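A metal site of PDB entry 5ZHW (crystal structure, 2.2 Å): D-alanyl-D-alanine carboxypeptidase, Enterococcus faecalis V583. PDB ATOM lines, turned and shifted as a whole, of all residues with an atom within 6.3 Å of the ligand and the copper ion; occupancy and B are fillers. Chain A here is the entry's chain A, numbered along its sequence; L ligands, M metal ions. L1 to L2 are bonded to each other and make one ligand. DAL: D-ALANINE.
Three residues have an atom within 4 Å of the copper ion: His 140, Asp 147 and His 193. The nearest printed residue that does not touch the copper ion is Arg 98 (4.2 Å).
OG of Ser 138 is in hydrogen-bond range of OXT of DAL L1 (2.5 Å). An oxygen (O) of DAL L1 sits close to the side-chain amide oxygen (OE1) of Gln 103 (3.0 Å). The backbone carbonyl oxygen (O) of Trp 131 is in hydrogen-bond range of a nitrogen (N) of DAL L1. The backbone NH (N) of Ala 133 lies within hydrogen-bond range of an oxygen (O) of DAL L1 (3.1 Å). An oxygen (O) of DAL L1 is in salt-bridge range of the guanidinium group (NH1) of Arg 98 (3.7 Å).
The side-chain carboxylate of Glu 190 lies close to an oxygen (O) of DAL L2 (3.3 Å). Merely in contact with the ligand: Trp 192, Val 132, Tyr 177, Glu 139 and Ile 106. Hydrophobic or aromatic side chains that line the ligand: Ile 106, Val 132, Ala 133, His 140, Tyr 177 and His 193. Within 4 Å of the ligand: Arg 98, Gln 103, Ile 106, Trp 131, Val 132, Ala 133, Ser 138, Glu 139, His 140, Asp 147, Tyr 177, Glu 190, Trp 192 and His 193.
NH2 of Arg 98 is in salt-bridge range of OD2 of Asp 147 (2.9 Å). A ring nitrogen (NE2) of His 193 lies within hydrogen-bond range of the side-chain carboxylate of Glu 139 (2.8 Å). The backbone NH (N) of His 140 is in hydrogen-bond range of the side-chain hydroxyl (OG) of Ser 138 (2.9 Å). O of His 140 lies within hydrogen-bond range of N of Arg 98 (3.2 Å). The side-chain amide oxygen of Gln 103 lies close to the backbone carbonyl oxygen of Ala 133. NH1 of Arg 98 lies close to NE2 of Gln 103, 3.0 Å away. OG1 of Thr 130 sits close to NE1 of Trp 131 (3.4 Å). The guanidinium group (NE) of Arg 98 is in hydrogen-bond range of the side-chain hydroxyl (OG) of Ser 95 (3.0 Å).
The copper ion is bound by the side-chain carboxylate (OD1) of Asp 147 (1.9 Å), an oxygen (O) of DAL L2 (2.0 Å), a ring nitrogen (ND1) of His 193 (2.0 Å) and a ring nitrogen (NE2) of His 140 (2.1 Å). The copper ion has four donor atoms within binding distance. Slightly farther from the copper ion lies OD2 of Asp 147 (2.8 Å).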
ATOM      1  N   SER A  95      -0.525  -0.059 -21.951  1.00  0.00           N
ATOM      2  CA  SER A  95      -0.518   1.292 -21.396  1.00  0.00           C
ATOM      3  C   SER A  95       0.294   2.244 -22.265  1.00  0.00           C
ATOM      4  O   SER A  95       1.458   1.953 -22.566  1.00  0.00           O
ATOM      5  CB  SER A  95       0.056   1.258 -19.981  1.00  0.00           C
ATOM      6  OG  SER A  95      -0.024   2.527 -19.358  1.00  0.00           O
ATOM      7  N   ARG A  98      -0.359   8.516 -19.913  1.00  0.00           N
ATOM      8  CA  ARG A  98      -0.952   8.590 -18.596  1.00  0.00           C
ATOM      9  C   ARG A  98      -0.927  10.018 -18.127  1.00  0.00           C
ATOM     10  O   ARG A  98       0.053  10.729 -18.310  1.00  0.00           O
ATOM     11  CB  ARG A  98      -0.129   7.802 -17.595  1.00  0.00           C
ATOM     12  CG  ARG A  98      -0.125   6.312 -17.827  1.00  0.00           C
ATOM     13  CD  ARG A  98       0.910   5.680 -16.901  1.00  0.00           C
ATOM     14  NE  ARG A  98       1.171   4.301 -17.257  1.00  0.00           N
ATOM     15  CZ  ARG A  98       2.198   3.589 -16.843  1.00  0.00           C
ATOM     16  NH1 ARG A  98       3.094   4.117 -16.012  1.00  0.00           N
ATOM     17  NH2 ARG A  98       2.330   2.339 -17.251  1.00  0.00           N
ATOM     18  N   GLN A 103      -0.608   8.264 -13.135  1.00  0.00           N
ATOM     19  CA  GLN A 103       0.736   7.860 -12.735  1.00  0.00           C
ATOM     20  C   GLN A 103       0.831   7.690 -11.228  1.00  0.00           C
ATOM     21  O   GLN A 103       1.448   6.727 -10.725  1.00  0.00           O
ATOM     22  CB  GLN A 103       1.784   8.864 -13.224  1.00  0.00           C
ATOM     23  CG  GLN A 103       3.236   8.397 -13.039  1.00  0.00           C
ATOM     24  CD  GLN A 103       3.607   7.111 -13.770  1.00  0.00           C
ATOM     25  OE1 GLN A 103       4.503   6.378 -13.362  1.00  0.00           O
ATOM     26  NE2 GLN A 103       2.946   6.854 -14.866  1.00  0.00           N
ATOM     27  N   ILE A 106      -0.941   4.492 -10.232  1.00  0.00           N
ATOM     28  CA  ILE A 106      -0.185   3.305 -10.579  1.00  0.00           C
ATOM     29  C   ILE A 106       0.917   3.126  -9.564  1.00  0.00           C
ATOM     30  O   ILE A 106       1.154   2.058  -9.130  1.00  0.00           O
ATOM     31  CB  ILE A 106       0.358   3.352 -12.005  1.00  0.00           C
ATOM     32  CG1 ILE A 106      -0.772   3.228 -13.003  1.00  0.00           C
ATOM     33  CG2 ILE A 106       1.358   2.241 -12.239  1.00  0.00           C
ATOM     34  CD1 ILE A 106      -0.321   3.347 -14.414  1.00  0.00           C
ATOM     35  N   LYS A 110       1.621   0.186  -6.632  1.00  0.00           N
ATOM     36  CA  LYS A 110       2.910  -0.499  -6.468  1.00  0.00           C
ATOM     37  C   LYS A 110       3.419  -0.380  -5.024  1.00  0.00           C
ATOM     38  O   LYS A 110       3.929  -1.355  -4.477  1.00  0.00           O
ATOM     39  CB  LYS A 110       3.941   0.013  -7.481  1.00  0.00           C
ATOM     40  CG  LYS A 110       5.308  -0.684  -7.453  1.00  0.00           C
ATOM     41  CD  LYS A 110       5.235  -2.188  -7.739  1.00  0.00           C
ATOM     42  CE  LYS A 110       4.781  -2.507  -9.157  1.00  0.00           C
ATOM     43  NZ  LYS A 110       4.926  -3.962  -9.449  1.00  0.00           N
ATOM     44  N   GLU A 129       9.629   2.980  -6.625  1.00  0.00           N
ATOM     45  CA  GLU A 129      10.288   3.856  -7.594  1.00  0.00           C
ATOM     46  C   GLU A 129      11.189   3.115  -8.589  1.00  0.00           C
ATOM     47  O   GLU A 129      11.375   3.596  -9.700  1.00  0.00           O
ATOM     48  CB  GLU A 129      11.115   4.945  -6.909  1.00  0.00           C
ATOM     49  CG  GLU A 129      10.301   6.079  -6.324  1.00  0.00           C
ATOM     50  CD  GLU A 129      11.095   7.384  -6.249  1.00  0.00           C
ATOM     51  OE1 GLU A 129      11.292   7.875  -5.108  1.00  0.00           O
ATOM     52  OE2 GLU A 129      11.509   7.912  -7.309  1.00  0.00           O
ATOM     53  N   THR A 130      11.716   1.963  -8.199  1.00  0.00           N
ATOM     54  CA  THR A 130      12.477   1.149  -9.137  1.00  0.00           C
ATOM     55  C   THR A 130      11.613   0.531 -10.255  1.00  0.00           C
ATOM     56  O   THR A 130      12.172   0.027 -11.226  1.00  0.00           O
ATOM     57  CB  THR A 130      13.280   0.018  -8.433  1.00  0.00           C
ATOM     58  OG1 THR A 130      12.404  -0.977  -7.920  1.00  0.00           O
ATOM     59  CG2 THR A 130      14.140   0.579  -7.295  1.00  0.00           C
ATOM     60  N   TRP A 131      10.284   0.559 -10.106  1.00  0.00           N
ATOM     61  CA  TRP A 131       9.334   0.020 -11.095  1.00  0.00           C
ATOM     62  C   TRP A 131       8.413   1.067 -11.698  1.00  0.00           C
ATOM     63  O   TRP A 131       8.079   0.985 -12.878  1.00  0.00           O
ATOM     64  CB  TRP A 131       8.471  -1.057 -10.444  1.00  0.00           C
ATOM     65  CG  TRP A 131       9.239  -2.232 -10.001  1.00  0.00           C
ATOM     66  CD1 TRP A 131       9.733  -2.476  -8.738  1.00  0.00           C
ATOM     67  CD2 TRP A 131       9.647  -3.344 -10.807  1.00  0.00           C
ATOM     68  NE1 TRP A 131      10.416  -3.660  -8.713  1.00  0.00           N
ATOM     69  CE2 TRP A 131      10.386  -4.220  -9.971  1.00  0.00           C
ATOM     70  CE3 TRP A 131       9.468  -3.682 -12.156  1.00  0.00           C
ATOM     71  CZ2 TRP A 131      10.935  -5.424 -10.437  1.00  0.00           C
ATOM     72  CZ3 TRP A 131      10.012  -4.883 -12.629  1.00  0.00           C
ATOM     73  CH2 TRP A 131      10.741  -5.740 -11.768  1.00  0.00           C
ATOM     74  N   VAL A 132       7.971   2.022 -10.891  1.00  0.00           N
ATOM     75  CA  VAL A 132       7.019   3.042 -11.328  1.00  0.00           C
ATOM     76  C   VAL A 132       7.591   4.394 -10.952  1.00  0.00           C
ATOM     77  O   VAL A 132       7.914   4.625  -9.795  1.00  0.00           O
ATOM     78  CB  VAL A 132       5.638   2.816 -10.690  1.00  0.00           C
ATOM     79  CG1 VAL A 132       4.600   3.811 -11.244  1.00  0.00           C
ATOM     80  CG2 VAL A 132       5.177   1.378 -10.921  1.00  0.00           C
ATOM     81  N   ALA A 133       7.718   5.281 -11.941  1.00  0.00           N
ATOM     82  CA  ALA A 133       8.283   6.613 -11.734  1.00  0.00           C
ATOM     83  C   ALA A 133       7.320   7.509 -10.982  1.00  0.00           C
ATOM     84  O   ALA A 133       6.084   7.327 -11.081  1.00  0.00           O
ATOM     85  CB  ALA A 133       8.679   7.228 -13.069  1.00  0.00           C
ATOM     86  N   VAL A 134       7.853   8.461 -10.207  1.00  0.00           N
ATOM     87  CA  VAL A 134       6.971   9.420  -9.514  1.00  0.00           C
ATOM     88  C   VAL A 134       6.358  10.291 -10.604  1.00  0.00           C
ATOM     89  O   VAL A 134       6.992  10.498 -11.636  1.00  0.00           O
ATOM     90  CB  VAL A 134       7.650  10.288  -8.399  1.00  0.00           C
ATOM     91  CG1 VAL A 134       8.259   9.395  -7.313  1.00  0.00           C
ATOM     92  CG2 VAL A 134       8.704  11.237  -8.939  1.00  0.00           C
ATOM     93  N   THR A 137       7.846  12.304 -13.895  1.00  0.00           N
ATOM     94  CA  THR A 137       9.087  11.678 -14.354  1.00  0.00           C
ATOM     95  C   THR A 137       8.875  10.386 -15.114  1.00  0.00           C
ATOM     96  O   THR A 137       9.854   9.693 -15.389  1.00  0.00           O
ATOM     97  CB  THR A 137      10.061  11.426 -13.174  1.00  0.00           C
ATOM     98  OG1 THR A 137       9.552  10.422 -12.295  1.00  0.00           O
ATOM     99  CG2 THR A 137      10.318  12.713 -12.397  1.00  0.00           C
ATOM    100  N   SER A 138       7.632  10.068 -15.505  1.00  0.00           N
ATOM    101  CA  SER A 138       7.379   8.906 -16.339  1.00  0.00           C
ATOM    102  C   SER A 138       7.428   9.297 -17.798  1.00  0.00           C
ATOM    103  O   SER A 138       6.854  10.324 -18.191  1.00  0.00           O
ATOM    104  CB  SER A 138       6.013   8.275 -16.046  1.00  0.00           C
ATOM    105  OG  SER A 138       5.746   7.191 -16.918  1.00  0.00           O
ATOM    106  N   GLU A 139       8.060   8.457 -18.591  1.00  0.00           N
ATOM    107  CA  GLU A 139       7.937   8.554 -20.043  1.00  0.00           C
ATOM    108  C   GLU A 139       6.513   8.361 -20.502  1.00  0.00           C
ATOM    109  O   GLU A 139       6.190   8.804 -21.591  1.00  0.00           O
ATOM    110  CB  GLU A 139       8.782   7.498 -20.749  1.00  0.00           C
ATOM    111  CG  GLU A 139      10.261   7.714 -20.652  1.00  0.00           C
ATOM    112  CD  GLU A 139      11.059   6.739 -21.499  1.00  0.00           C
ATOM    113  OE1 GLU A 139      10.573   5.593 -21.715  1.00  0.00           O
ATOM    114  OE2 GLU A 139      12.143   7.137 -21.939  1.00  0.00           O
ATOM    115  N   HIS A 140       5.671   7.673 -19.729  1.00  0.00           N
ATOM    116  CA  HIS A 140       4.278   7.523 -20.141  1.00  0.00           C
ATOM    117  C   HIS A 140       3.541   8.856 -20.250  1.00  0.00           C
ATOM    118  O   HIS A 140       2.636   9.006 -21.043  1.00  0.00           O
ATOM    119  CB  HIS A 140       3.539   6.575 -19.232  1.00  0.00           C
ATOM    120  CG  HIS A 140       3.921   5.163 -19.443  1.00  0.00           C
ATOM    121  ND1 HIS A 140       3.279   4.368 -20.363  1.00  0.00           N
ATOM    122  CD2 HIS A 140       4.901   4.419 -18.906  1.00  0.00           C
ATOM    123  CE1 HIS A 140       3.848   3.172 -20.365  1.00  0.00           C
ATOM    124  NE2 HIS A 140       4.834   3.178 -19.492  1.00  0.00           N
ATOM    125  N   ALA A 145       5.992   6.555 -24.766  1.00  0.00           N
ATOM    126  CA  ALA A 145       6.272   5.201 -24.255  1.00  0.00           C
ATOM    127  C   ALA A 145       4.998   4.355 -24.290  1.00  0.00           C
ATOM    128  O   ALA A 145       3.911   4.833 -23.983  1.00  0.00           O
ATOM    129  CB  ALA A 145       6.789   5.278 -22.820  1.00  0.00           C
ATOM    130  N   VAL A 146       5.168   3.094 -24.651  1.00  0.00           N
ATOM    131  CA  VAL A 146       4.090   2.104 -24.572  1.00  0.00           C
ATOM    132  C   VAL A 146       4.581   0.895 -23.807  1.00  0.00           C
ATOM    133  O   VAL A 146       5.743   0.484 -23.974  1.00  0.00           O
ATOM    134  CB  VAL A 146       3.569   1.677 -25.947  1.00  0.00           C
ATOM    135  CG1 VAL A 146       2.779   2.814 -26.594  1.00  0.00           C
ATOM    136  CG2 VAL A 146       4.661   1.221 -26.876  1.00  0.00           C
ATOM    137  N   ASP A 147       3.700   0.346 -22.953  1.00  0.00           N
ATOM    138  CA  ASP A 147       3.904  -0.953 -22.367  1.00  0.00           C
ATOM    139  C   ASP A 147       3.182  -1.921 -23.259  1.00  0.00           C
ATOM    140  O   ASP A 147       1.979  -1.811 -23.474  1.00  0.00           O
ATOM    141  CB  ASP A 147       3.335  -1.043 -20.952  1.00  0.00           C
ATOM    142  CG  ASP A 147       4.062  -0.145 -19.988  1.00  0.00           C
ATOM    143  OD1 ASP A 147       5.241   0.183 -20.215  1.00  0.00           O
ATOM    144  OD2 ASP A 147       3.443   0.245 -18.994  1.00  0.00           O
ATOM    145  N   TYR A 177      14.477  -0.011 -20.531  1.00  0.00           N
ATOM    146  CA  TYR A 177      15.021  -0.368 -19.231  1.00  0.00           C
ATOM    147  C   TYR A 177      15.545  -1.812 -19.273  1.00  0.00           C
ATOM    148  O   TYR A 177      14.927  -2.748 -18.764  1.00  0.00           O
ATOM    149  CB  TYR A 177      13.965  -0.175 -18.121  1.00  0.00           C
ATOM    150  CG  TYR A 177      13.334   1.195 -18.085  1.00  0.00           C
ATOM    151  CD1 TYR A 177      14.091   2.335 -17.831  1.00  0.00           C
ATOM    152  CD2 TYR A 177      11.950   1.364 -18.305  1.00  0.00           C
ATOM    153  CE1 TYR A 177      13.506   3.603 -17.802  1.00  0.00           C
ATOM    154  CE2 TYR A 177      11.365   2.609 -18.259  1.00  0.00           C
ATOM    155  CZ  TYR A 177      12.145   3.745 -18.010  1.00  0.00           C
ATOM    156  OH  TYR A 177      11.566   5.008 -17.987  1.00  0.00           O
ATOM    157  N   VAL A 187      16.076   1.856 -13.106  1.00  0.00           N
ATOM    158  CA  VAL A 187      14.802   1.169 -13.258  1.00  0.00           C
ATOM    159  C   VAL A 187      15.084  -0.300 -13.511  1.00  0.00           C
ATOM    160  O   VAL A 187      16.038  -0.661 -14.217  1.00  0.00           O
ATOM    161  CB  VAL A 187      13.960   1.791 -14.413  1.00  0.00           C
ATOM    162  CG1 VAL A 187      12.658   1.022 -14.629  1.00  0.00           C
ATOM    163  CG2 VAL A 187      13.671   3.276 -14.163  1.00  0.00           C
ATOM    164  N   GLU A 190      12.135  -4.179 -17.217  1.00  0.00           N
ATOM    165  CA  GLU A 190      10.753  -4.028 -17.662  1.00  0.00           C
ATOM    166  C   GLU A 190      10.703  -4.353 -19.161  1.00  0.00           C
ATOM    167  O   GLU A 190      10.769  -3.440 -20.008  1.00  0.00           O
ATOM    168  CB  GLU A 190      10.298  -2.611 -17.385  1.00  0.00           C
ATOM    169  CG  GLU A 190      10.217  -2.332 -15.889  1.00  0.00           C
ATOM    170  CD  GLU A 190       9.662  -0.955 -15.557  1.00  0.00           C
ATOM    171  OE1 GLU A 190       9.401  -0.145 -16.484  1.00  0.00           O
ATOM    172  OE2 GLU A 190       9.479  -0.714 -14.362  1.00  0.00           O
ATOM    173  N   TRP A 192       8.458  -5.167 -21.078  1.00  0.00           N
ATOM    174  CA  TRP A 192       7.283  -4.568 -21.738  1.00  0.00           C
ATOM    175  C   TRP A 192       7.406  -3.075 -22.133  1.00  0.00           C
ATOM    176  O   TRP A 192       6.647  -2.616 -22.973  1.00  0.00           O
ATOM    177  CB  TRP A 192       6.041  -4.748 -20.847  1.00  0.00           C
ATOM    178  CG  TRP A 192       6.264  -4.233 -19.472  1.00  0.00           C
ATOM    179  CD1 TRP A 192       6.195  -2.963 -19.062  1.00  0.00           C
ATOM    180  CD2 TRP A 192       6.662  -5.009 -18.334  1.00  0.00           C
ATOM    181  NE1 TRP A 192       6.515  -2.863 -17.749  1.00  0.00           N
ATOM    182  CE2 TRP A 192       6.804  -4.117 -17.270  1.00  0.00           C
ATOM    183  CE3 TRP A 192       6.906  -6.359 -18.104  1.00  0.00           C
ATOM    184  CZ2 TRP A 192       7.177  -4.531 -15.975  1.00  0.00           C
ATOM    185  CZ3 TRP A 192       7.274  -6.782 -16.822  1.00  0.00           C
ATOM    186  CH2 TRP A 192       7.399  -5.869 -15.775  1.00  0.00           C
ATOM    187  N   HIS A 193       8.323  -2.315 -21.548  1.00  0.00           N
ATOM    188  CA  HIS A 193       8.337  -0.854 -21.724  1.00  0.00           C
ATOM    189  C   HIS A 193       9.252  -0.421 -22.878  1.00  0.00           C
ATOM    190  O   HIS A 193      10.479  -0.520 -22.790  1.00  0.00           O
ATOM    191  CB  HIS A 193       8.736  -0.161 -20.430  1.00  0.00           C
ATOM    192  CG  HIS A 193       8.678   1.344 -20.488  1.00  0.00           C
ATOM    193  ND1 HIS A 193       7.753   2.081 -19.772  1.00  0.00           N
ATOM    194  CD2 HIS A 193       9.473   2.239 -21.123  1.00  0.00           C
ATOM    195  CE1 HIS A 193       7.980   3.364 -19.987  1.00  0.00           C
ATOM    196  NE2 HIS A 193       9.010   3.496 -20.800  1.00  0.00           N
ATOM    197  N   TYR A 194       8.618   0.085 -23.929  1.00  0.00           N
ATOM    198  CA  TYR A 194       9.276   0.526 -25.142  1.00  0.00           C
ATOM    199  C   TYR A 194       9.076   2.039 -25.367  1.00  0.00           C
ATOM    200  O   TYR A 194       7.977   2.553 -25.179  1.00  0.00           O
ATOM    201  CB  TYR A 194       8.809  -0.331 -26.337  1.00  0.00           C
ATOM    202  CG  TYR A 194       9.589  -1.603 -26.325  1.00  0.00           C
ATOM    203  CD1 TYR A 194       9.261  -2.653 -25.436  1.00  0.00           C
ATOM    204  CD2 TYR A 194      10.748  -1.718 -27.067  1.00  0.00           C
ATOM    205  CE1 TYR A 194      10.049  -3.795 -25.366  1.00  0.00           C
ATOM    206  CE2 TYR A 194      11.535  -2.847 -26.991  1.00  0.00           C
ATOM    207  CZ  TYR A 194      11.186  -3.887 -26.148  1.00  0.00           C
ATOM    208  OH  TYR A 194      12.033  -4.976 -26.138  1.00  0.00           O
HETATM  209  N   DAL L   1       6.711   1.958 -15.425  1.00  0.00           N
HETATM  210  CA  DAL L   1       7.686   2.970 -15.962  1.00  0.00           C
HETATM  211  CB  DAL L   1       9.047   2.913 -15.222  1.00  0.00           C
HETATM  212  C   DAL L   1       7.108   4.366 -15.748  1.00  0.00           C
HETATM  213  O   DAL L   1       6.535   4.586 -14.710  1.00  0.00           O
HETATM  214  OXT DAL L   1       7.315   5.223 -16.601  1.00  0.00           O
HETATM  215  N   DAL L   2       4.130   0.836 -14.661  1.00  0.00           N
HETATM  216  CA  DAL L   2       5.167   0.039 -15.363  1.00  0.00           C
HETATM  217  CB  DAL L   2       5.925  -0.914 -14.418  1.00  0.00           C
HETATM  218  C   DAL L   2       6.143   0.938 -16.137  1.00  0.00           C
HETATM  219  O   DAL L   2       6.356   0.679 -17.321  1.00  0.00           O
HETATM  220 CU    CU M   1       5.982   1.528 -19.051  1.00  0.00          CU
